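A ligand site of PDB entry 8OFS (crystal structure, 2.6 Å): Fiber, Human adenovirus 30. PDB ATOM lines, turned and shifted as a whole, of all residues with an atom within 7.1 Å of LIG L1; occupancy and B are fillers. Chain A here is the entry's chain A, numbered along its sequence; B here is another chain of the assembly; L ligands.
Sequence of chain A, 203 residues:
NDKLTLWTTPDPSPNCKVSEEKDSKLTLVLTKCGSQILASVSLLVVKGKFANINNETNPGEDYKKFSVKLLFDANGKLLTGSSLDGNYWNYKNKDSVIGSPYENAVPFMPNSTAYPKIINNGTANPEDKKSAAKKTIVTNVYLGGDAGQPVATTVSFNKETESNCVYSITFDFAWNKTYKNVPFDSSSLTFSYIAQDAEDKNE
CA of Gly 148 touches O8 of LIG L1, at 3.4 Å.
Pro 150 of chain A touches LIG L1 (CB to O4, 3.3 Å).
CG1 of Val 138 of chain B touches C11 of LIG L1, 3.7 Å away.
Thr 139 of chain B touches LIG L1 (O to C11, 3.5 Å).
Ala 152 of chain B touches LIG L1.
ND2 of Asn 176 of chain B touches C9 of LIG L1, at 3.6 Å.
Hydrophobic or aromatic side chains within 4 Å of LIG L1: Tyr 142 of chain A, Ala 147, Pro 150 of chain A, Val 138 of chain B and Ala 152 of chain B.
Of the 22 residues printed, 10 come within 4 Å of LIG L1.
ND2 of Asn 140 of chain B sits close to N of Ala 152 of chain B (3.3 Å).
NZ of Lys 177 lies within hydrogen-bond range of O of Gly 148, at 3.4 Å.
OD1 of Asp 146 sits at hydrogen-bond distance from N of Gly 148, at 2.8 Å.
The backbone NH (N) of Thr 139 of chain B lies within hydrogen-bond range of the backbone carbonyl oxygen (O) of Thr 153 of chain B, 2.9 Å away.
N of Ala 152 of chain B sits at hydrogen-bond distance from O of Ala 174 of chain B, at 2.9 Å.
N1 of LIG L1 is in hydrogen-bond range of O of Ala 147, 2.7 Å away.
OD1 of Asn 140 of chain B sits close to O9 of LIG L1 (2.8 Å).
An oxygen (O4) of LIG L1 sits at hydrogen-bond distance from the side-chain hydroxyl of Tyr 142 of chain A (2.9 Å).
An oxygen (O1) of LIG L1 lies within salt-bridge range of the side-chain amino group (NZ) of Lys 177.
The side-chain amide oxygen (OD1) of Asn 140 of chain A lies close to an oxygen (O9) of LG2 L2.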
ATOM      1  N   ASN A 140     -10.675  12.539  22.375  1.00  0.00           N
ATOM      2  CA  ASN A 140     -12.096  12.754  22.027  1.00  0.00           C
ATOM      3  C   ASN A 140     -12.203  13.081  20.542  1.00  0.00           C
ATOM      4  O   ASN A 140     -11.353  13.856  20.042  1.00  0.00           O
ATOM      5  CB  ASN A 140     -12.714  13.899  22.808  1.00  0.00           C
ATOM      6  CG  ASN A 140     -12.908  13.582  24.272  1.00  0.00           C
ATOM      7  OD1 ASN A 140     -12.155  14.076  25.111  1.00  0.00           O
ATOM      8  ND2 ASN A 140     -13.907  12.761  24.579  1.00  0.00           N
ATOM      9  N   VAL A 141     -13.258  12.581  19.891  1.00  0.00           N
ATOM     10  CA  VAL A 141     -13.839  13.188  18.674  1.00  0.00           C
ATOM     11  C   VAL A 141     -15.141  13.882  19.067  1.00  0.00           C
ATOM     12  O   VAL A 141     -15.575  13.735  20.228  1.00  0.00           O
ATOM     13  CB  VAL A 141     -14.037  12.161  17.555  1.00  0.00           C
ATOM     14  CG1 VAL A 141     -12.718  11.551  17.148  1.00  0.00           C
ATOM     15  CG2 VAL A 141     -15.045  11.087  17.941  1.00  0.00           C
ATOM     16  N   TYR A 142     -15.698  14.650  18.136  1.00  0.00           N
ATOM     17  CA  TYR A 142     -16.797  15.605  18.393  1.00  0.00           C
ATOM     18  C   TYR A 142     -17.838  15.462  17.287  1.00  0.00           C
ATOM     19  O   TYR A 142     -17.538  15.772  16.124  1.00  0.00           O
ATOM     20  CB  TYR A 142     -16.211  17.006  18.543  1.00  0.00           C
ATOM     21  CG  TYR A 142     -15.491  17.178  19.839  1.00  0.00           C
ATOM     22  CD1 TYR A 142     -16.180  17.513  20.980  1.00  0.00           C
ATOM     23  CD2 TYR A 142     -14.140  16.912  19.952  1.00  0.00           C
ATOM     24  CE1 TYR A 142     -15.549  17.640  22.196  1.00  0.00           C
ATOM     25  CE2 TYR A 142     -13.478  17.044  21.167  1.00  0.00           C
ATOM     26  CZ  TYR A 142     -14.194  17.401  22.294  1.00  0.00           C
ATOM     27  OH  TYR A 142     -13.590  17.536  23.498  1.00  0.00           O
ATOM     28  N   ASP A 146     -19.346  19.786  16.402  1.00  0.00           N
ATOM     29  CA  ASP A 146     -19.786  20.610  17.551  1.00  0.00           C
ATOM     30  C   ASP A 146     -18.929  20.256  18.784  1.00  0.00           C
ATOM     31  O   ASP A 146     -18.847  19.055  19.142  1.00  0.00           O
ATOM     32  CB  ASP A 146     -21.282  20.419  17.808  1.00  0.00           C
ATOM     33  CG  ASP A 146     -21.867  21.334  18.883  1.00  0.00           C
ATOM     34  OD1 ASP A 146     -21.070  21.895  19.670  1.00  0.00           O
ATOM     35  OD2 ASP A 146     -23.090  21.476  18.921  1.00  0.00           O
ATOM     36  N   ALA A 147     -18.320  21.277  19.404  1.00  0.00           N
ATOM     37  CA  ALA A 147     -17.428  21.161  20.577  1.00  0.00           C
ATOM     38  C   ALA A 147     -18.218  20.696  21.812  1.00  0.00           C
ATOM     39  O   ALA A 147     -17.580  20.314  22.795  1.00  0.00           O
ATOM     40  CB  ALA A 147     -16.763  22.503  20.830  1.00  0.00           C
ATOM     41  N   GLY A 148     -19.542  20.785  21.775  1.00  0.00           N
ATOM     42  CA  GLY A 148     -20.418  20.415  22.896  1.00  0.00           C
ATOM     43  C   GLY A 148     -20.831  18.950  22.839  1.00  0.00           C
ATOM     44  O   GLY A 148     -21.639  18.541  23.701  1.00  0.00           O
ATOM     45  N   GLN A 149     -20.309  18.189  21.869  1.00  0.00           N
ATOM     46  CA  GLN A 149     -20.769  16.805  21.541  1.00  0.00           C
ATOM     47  C   GLN A 149     -19.560  15.857  21.513  1.00  0.00           C
ATOM     48  O   GLN A 149     -19.256  15.228  20.490  1.00  0.00           O
ATOM     49  CB  GLN A 149     -21.588  16.836  20.233  1.00  0.00           C
ATOM     50  CG  GLN A 149     -22.677  17.905  20.250  1.00  0.00           C
ATOM     51  CD  GLN A 149     -23.851  17.570  19.363  1.00  0.00           C
ATOM     52  OE1 GLN A 149     -23.699  17.216  18.202  1.00  0.00           O
ATOM     53  NE2 GLN A 149     -25.052  17.694  19.924  1.00  0.00           N
ATOM     54  N   PRO A 150     -18.881  15.681  22.663  1.00  0.00           N
ATOM     55  CA  PRO A 150     -17.716  14.802  22.776  1.00  0.00           C
ATOM     56  C   PRO A 150     -18.034  13.299  22.846  1.00  0.00           C
ATOM     57  O   PRO A 150     -18.897  12.892  23.625  1.00  0.00           O
ATOM     58  CB  PRO A 150     -17.100  15.236  24.101  1.00  0.00           C
ATOM     59  CG  PRO A 150     -18.273  15.670  24.923  1.00  0.00           C
ATOM     60  CD  PRO A 150     -19.168  16.371  23.931  1.00  0.00           C
ATOM     61  N   VAL A 151     -17.277  12.515  22.079  1.00  0.00           N
ATOM     62  CA  VAL A 151     -17.167  11.031  22.215  1.00  0.00           C
ATOM     63  C   VAL A 151     -15.750  10.690  22.653  1.00  0.00           C
ATOM     64  O   VAL A 151     -14.813  11.009  21.890  1.00  0.00           O
ATOM     65  CB  VAL A 151     -17.515  10.319  20.899  1.00  0.00           C
ATOM     66  CG1 VAL A 151     -17.281   8.814  21.016  1.00  0.00           C
ATOM     67  CG2 VAL A 151     -18.930  10.624  20.441  1.00  0.00           C
ATOM     68  N   LYS A 177     -22.908  11.932  27.926  1.00  0.00           N
ATOM     69  CA  LYS A 177     -24.003  12.842  27.508  1.00  0.00           C
ATOM     70  C   LYS A 177     -25.224  11.983  27.148  1.00  0.00           C
ATOM     71  O   LYS A 177     -25.020  10.848  26.671  1.00  0.00           O
ATOM     72  CB  LYS A 177     -23.585  13.711  26.305  1.00  0.00           C
ATOM     73  CG  LYS A 177     -22.290  14.491  26.466  1.00  0.00           C
ATOM     74  CD  LYS A 177     -22.459  15.894  26.998  1.00  0.00           C
ATOM     75  CE  LYS A 177     -21.126  16.589  27.255  1.00  0.00           C
ATOM     76  NZ  LYS A 177     -21.216  18.056  27.066  1.00  0.00           N
ATOM     77  N   VAL B 138     -12.012  19.241  15.963  1.00  0.00           N
ATOM     78  CA  VAL B 138     -12.315  19.919  17.258  1.00  0.00           C
ATOM     79  C   VAL B 138     -11.375  19.394  18.331  1.00  0.00           C
ATOM     80  O   VAL B 138     -11.281  18.146  18.507  1.00  0.00           O
ATOM     81  CB  VAL B 138     -13.789  19.737  17.669  1.00  0.00           C
ATOM     82  CG1 VAL B 138     -14.142  20.620  18.854  1.00  0.00           C
ATOM     83  CG2 VAL B 138     -14.729  19.991  16.519  1.00  0.00           C
ATOM     84  N   THR B 139     -10.773  20.311  19.062  1.00  0.00           N
ATOM     85  CA  THR B 139      -9.714  20.054  20.070  1.00  0.00           C
ATOM     86  C   THR B 139      -9.677  21.264  21.015  1.00  0.00           C
ATOM     87  O   THR B 139     -10.668  22.015  21.019  1.00  0.00           O
ATOM     88  CB  THR B 139      -8.390  19.741  19.344  1.00  0.00           C
ATOM     89  OG1 THR B 139      -7.504  19.088  20.239  1.00  0.00           O
ATOM     90  CG2 THR B 139      -7.721  20.973  18.802  1.00  0.00           C
ATOM     91  N   ASN B 140      -8.620  21.391  21.815  1.00  0.00           N
ATOM     92  CA  ASN B 140      -8.349  22.585  22.647  1.00  0.00           C
ATOM     93  C   ASN B 140      -6.895  23.015  22.468  1.00  0.00           C
ATOM     94  O   ASN B 140      -6.018  22.133  22.382  1.00  0.00           O
ATOM     95  CB  ASN B 140      -8.593  22.343  24.128  1.00  0.00           C
ATOM     96  CG  ASN B 140     -10.050  22.207  24.462  1.00  0.00           C
ATOM     97  OD1 ASN B 140     -10.505  21.120  24.730  1.00  0.00           O
ATOM     98  ND2 ASN B 140     -10.789  23.299  24.473  1.00  0.00           N
ATOM     99  N   TYR B 142      -4.377  25.970  24.787  1.00  0.00           N
ATOM    100  CA  TYR B 142      -4.275  26.414  26.195  1.00  0.00           C
ATOM    101  C   TYR B 142      -3.453  27.700  26.250  1.00  0.00           C
ATOM    102  O   TYR B 142      -2.245  27.694  25.902  1.00  0.00           O
ATOM    103  CB  TYR B 142      -3.721  25.275  27.037  1.00  0.00           C
ATOM    104  CG  TYR B 142      -4.736  24.169  27.236  1.00  0.00           C
ATOM    105  CD1 TYR B 142      -4.961  23.224  26.231  1.00  0.00           C
ATOM    106  CD2 TYR B 142      -5.542  24.128  28.352  1.00  0.00           C
ATOM    107  CE1 TYR B 142      -5.920  22.234  26.386  1.00  0.00           C
ATOM    108  CE2 TYR B 142      -6.493  23.138  28.523  1.00  0.00           C
ATOM    109  CZ  TYR B 142      -6.691  22.198  27.531  1.00  0.00           C
ATOM    110  OH  TYR B 142      -7.658  21.245  27.690  1.00  0.00           O
ATOM    111  N   PRO B 150      -8.201  26.814  28.825  1.00  0.00           N
ATOM    112  CA  PRO B 150      -8.582  26.197  27.549  1.00  0.00           C
ATOM    113  C   PRO B 150      -9.347  27.104  26.575  1.00  0.00           C
ATOM    114  O   PRO B 150     -10.297  27.770  26.985  1.00  0.00           O
ATOM    115  CB  PRO B 150      -9.511  25.056  27.989  1.00  0.00           C
ATOM    116  CG  PRO B 150     -10.161  25.597  29.251  1.00  0.00           C
ATOM    117  CD  PRO B 150      -9.049  26.371  29.939  1.00  0.00           C
ATOM    118  N   VAL B 151      -8.966  27.039  25.310  1.00  0.00           N
ATOM    119  CA  VAL B 151      -9.759  27.568  24.163  1.00  0.00           C
ATOM    120  C   VAL B 151     -10.184  26.389  23.280  1.00  0.00           C
ATOM    121  O   VAL B 151      -9.282  25.709  22.746  1.00  0.00           O
ATOM    122  CB  VAL B 151      -8.967  28.595  23.342  1.00  0.00           C
ATOM    123  CG1 VAL B 151      -9.726  29.028  22.097  1.00  0.00           C
ATOM    124  CG2 VAL B 151      -8.574  29.810  24.181  1.00  0.00           C
ATOM    125  N   ALA B 152     -11.482  26.184  23.136  1.00  0.00           N
ATOM    126  CA  ALA B 152     -12.072  25.281  22.126  1.00  0.00           C
ATOM    127  C   ALA B 152     -11.619  25.719  20.728  1.00  0.00           C
ATOM    128  O   ALA B 152     -11.923  26.839  20.337  1.00  0.00           O
ATOM    129  CB  ALA B 152     -13.575  25.264  22.253  1.00  0.00           C
ATOM    130  N   THR B 153     -10.882  24.867  20.046  1.00  0.00           N
ATOM    131  CA  THR B 153     -10.242  25.141  18.747  1.00  0.00           C
ATOM    132  C   THR B 153     -10.841  24.222  17.678  1.00  0.00           C
ATOM    133  O   THR B 153     -10.886  22.990  17.892  1.00  0.00           O
ATOM    134  CB  THR B 153      -8.723  24.978  18.859  1.00  0.00           C
ATOM    135  OG1 THR B 153      -8.250  25.853  19.884  1.00  0.00           O
ATOM    136  CG2 THR B 153      -7.992  25.246  17.563  1.00  0.00           C
ATOM    137  N   THR B 154     -11.293  24.797  16.573  1.00  0.00           N
ATOM    138  CA  THR B 154     -11.978  24.088  15.474  1.00  0.00           C
ATOM    139  C   THR B 154     -11.260  24.428  14.158  1.00  0.00           C
ATOM    140  O   THR B 154     -11.488  25.548  13.631  1.00  0.00           O
ATOM    141  CB  THR B 154     -13.467  24.450  15.475  1.00  0.00           C
ATOM    142  OG1 THR B 154     -13.899  24.485  16.840  1.00  0.00           O
ATOM    143  CG2 THR B 154     -14.307  23.474  14.687  1.00  0.00           C
ATOM    144  N   ALA B 174     -12.969  29.713  20.691  1.00  0.00           N
ATOM    145  CA  ALA B 174     -14.033  30.136  21.627  1.00  0.00           C
ATOM    146  C   ALA B 174     -13.747  29.599  23.024  1.00  0.00           C
ATOM    147  O   ALA B 174     -13.072  28.577  23.107  1.00  0.00           O
ATOM    148  CB  ALA B 174     -15.376  29.670  21.109  1.00  0.00           C
ATOM    149  N   TRP B 175     -14.258  30.262  24.072  1.00  0.00           N
ATOM    150  CA  TRP B 175     -14.039  29.864  25.487  1.00  0.00           C
ATOM    151  C   TRP B 175     -15.237  30.250  26.371  1.00  0.00           C
ATOM    152  O   TRP B 175     -15.927  31.218  26.035  1.00  0.00           O
ATOM    153  CB  TRP B 175     -12.724  30.459  26.025  1.00  0.00           C
ATOM    154  CG  TRP B 175     -12.571  31.941  25.853  1.00  0.00           C
ATOM    155  CD1 TRP B 175     -12.905  32.916  26.750  1.00  0.00           C
ATOM    156  CD2 TRP B 175     -11.965  32.618  24.735  1.00  0.00           C
ATOM    157  NE1 TRP B 175     -12.572  34.154  26.260  1.00  0.00           N
ATOM    158  CE2 TRP B 175     -11.999  34.001  25.027  1.00  0.00           C
ATOM    159  CE3 TRP B 175     -11.420  32.197  23.520  1.00  0.00           C
ATOM    160  CZ2 TRP B 175     -11.503  34.958  24.138  1.00  0.00           C
ATOM    161  CZ3 TRP B 175     -10.928  33.141  22.645  1.00  0.00           C
ATOM    162  CH2 TRP B 175     -10.976  34.504  22.957  1.00  0.00           C
ATOM    163  N   ASN B 176     -15.461  29.487  27.442  1.00  0.00           N
ATOM    164  CA  ASN B 176     -16.576  29.673  28.420  1.00  0.00           C
ATOM    165  C   ASN B 176     -16.071  30.451  29.627  1.00  0.00           C
ATOM    166  O   ASN B 176     -16.863  31.170  30.238  1.00  0.00           O
ATOM    167  CB  ASN B 176     -17.132  28.343  28.936  1.00  0.00           C
ATOM    168  CG  ASN B 176     -17.997  27.625  27.926  1.00  0.00           C
ATOM    169  OD1 ASN B 176     -18.626  28.272  27.073  1.00  0.00           O
ATOM    170  ND2 ASN B 176     -18.052  26.298  28.004  1.00  0.00           N
HETATM  171  C1  LIG L   1     -18.399  20.223  28.828  1.00  0.00           C
HETATM  172  C2  LIG L   1     -17.905  20.076  27.371  1.00  0.00           C
HETATM  173  C3  LIG L   1     -17.081  18.819  27.137  1.00  0.00           C
HETATM  174  C4  LIG L   1     -16.490  18.781  25.738  1.00  0.00           C
HETATM  175  C5  LIG L   1     -15.783  20.101  25.445  1.00  0.00           C
HETATM  176  C6  LIG L   1     -16.760  21.253  25.654  1.00  0.00           C
HETATM  177  C7  LIG L   1     -16.190  22.622  25.290  1.00  0.00           C
HETATM  178  C8  LIG L   1     -17.248  23.509  24.564  1.00  0.00           C
HETATM  179  C9  LIG L   1     -18.484  23.784  25.401  1.00  0.00           C
HETATM  180  C10 LIG L   1     -13.989  20.657  23.893  1.00  0.00           C
HETATM  181  C11 LIG L   1     -13.488  20.595  22.478  1.00  0.00           C
HETATM  182  N1  LIG L   1     -15.183  20.128  24.125  1.00  0.00           N
HETATM  183  O1  LIG L   1     -19.135  19.377  29.301  1.00  0.00           O
HETATM  184  O2  LIG L   1     -18.085  21.191  29.481  1.00  0.00           O
HETATM  185  O3  LIG L   1     -19.019  20.043  26.521  1.00  0.00           O
HETATM  186  O4  LIG L   1     -15.583  17.692  25.601  1.00  0.00           O
HETATM  187  O5  LIG L   1     -17.147  21.258  27.042  1.00  0.00           O
HETATM  188  O6  LIG L   1     -15.707  23.273  26.468  1.00  0.00           O
HETATM  189  O7  LIG L   1     -16.647  24.740  24.160  1.00  0.00           O
HETATM  190  O8  LIG L   1     -19.591  22.981  24.996  1.00  0.00           O
HETATM  191  O9  LIG L   1     -13.345  21.200  24.781  1.00  0.00           O
HETATM  192  C1  LG2 L   2     -14.707  13.481  33.519  1.00  0.00           C
HETATM  193  C2  LG2 L   2     -14.007  12.595  32.486  1.00  0.00           C
HETATM  194  C3  LG2 L   2     -12.638  13.197  32.213  1.00  0.00           C
HETATM  195  C4  LG2 L   2     -11.897  12.512  31.073  1.00  0.00           C
HETATM  196  C5  LG2 L   2     -12.823  12.275  29.877  1.00  0.00           C
HETATM  197  C6  LG2 L   2     -14.142  11.617  30.305  1.00  0.00           C
HETATM  198  C7  LG2 L   2     -15.097  11.334  29.140  1.00  0.00           C
HETATM  199  C8  LG2 L   2     -15.769   9.909  29.271  1.00  0.00           C
HETATM  200  C9  LG2 L   2     -16.479   9.696  30.584  1.00  0.00           C
HETATM  201  C10 LG2 L   2     -11.597  12.043  27.769  1.00  0.00           C
HETATM  202  C11 LG2 L   2     -10.861  11.108  26.852  1.00  0.00           C
HETATM  203  N1  LG2 L   2     -12.120  11.496  28.862  1.00  0.00           N
HETATM  204  O1  LG2 L   2     -15.668  14.173  33.192  1.00  0.00           O
HETATM  205  O2  LG2 L   2     -14.271  13.503  34.659  1.00  0.00           O
HETATM  206  O3  LG2 L   2     -13.886  11.318  33.049  1.00  0.00           O
HETATM  207  O4  LG2 L   2     -10.780  13.296  30.674  1.00  0.00           O
HETATM  208  O5  LG2 L   2     -14.791  12.484  31.276  1.00  0.00           O
HETATM  209  O6  LG2 L   2     -16.084  12.373  29.041  1.00  0.00           O
HETATM  210  O7  LG2 L   2     -16.699   9.675  28.203  1.00  0.00           O
HETATM  211  O8  LG2 L   2     -15.557   9.661  31.674  1.00  0.00           O
HETATM  212  O9  LG2 L   2     -11.722  13.242  27.525  1.00  0.00           O
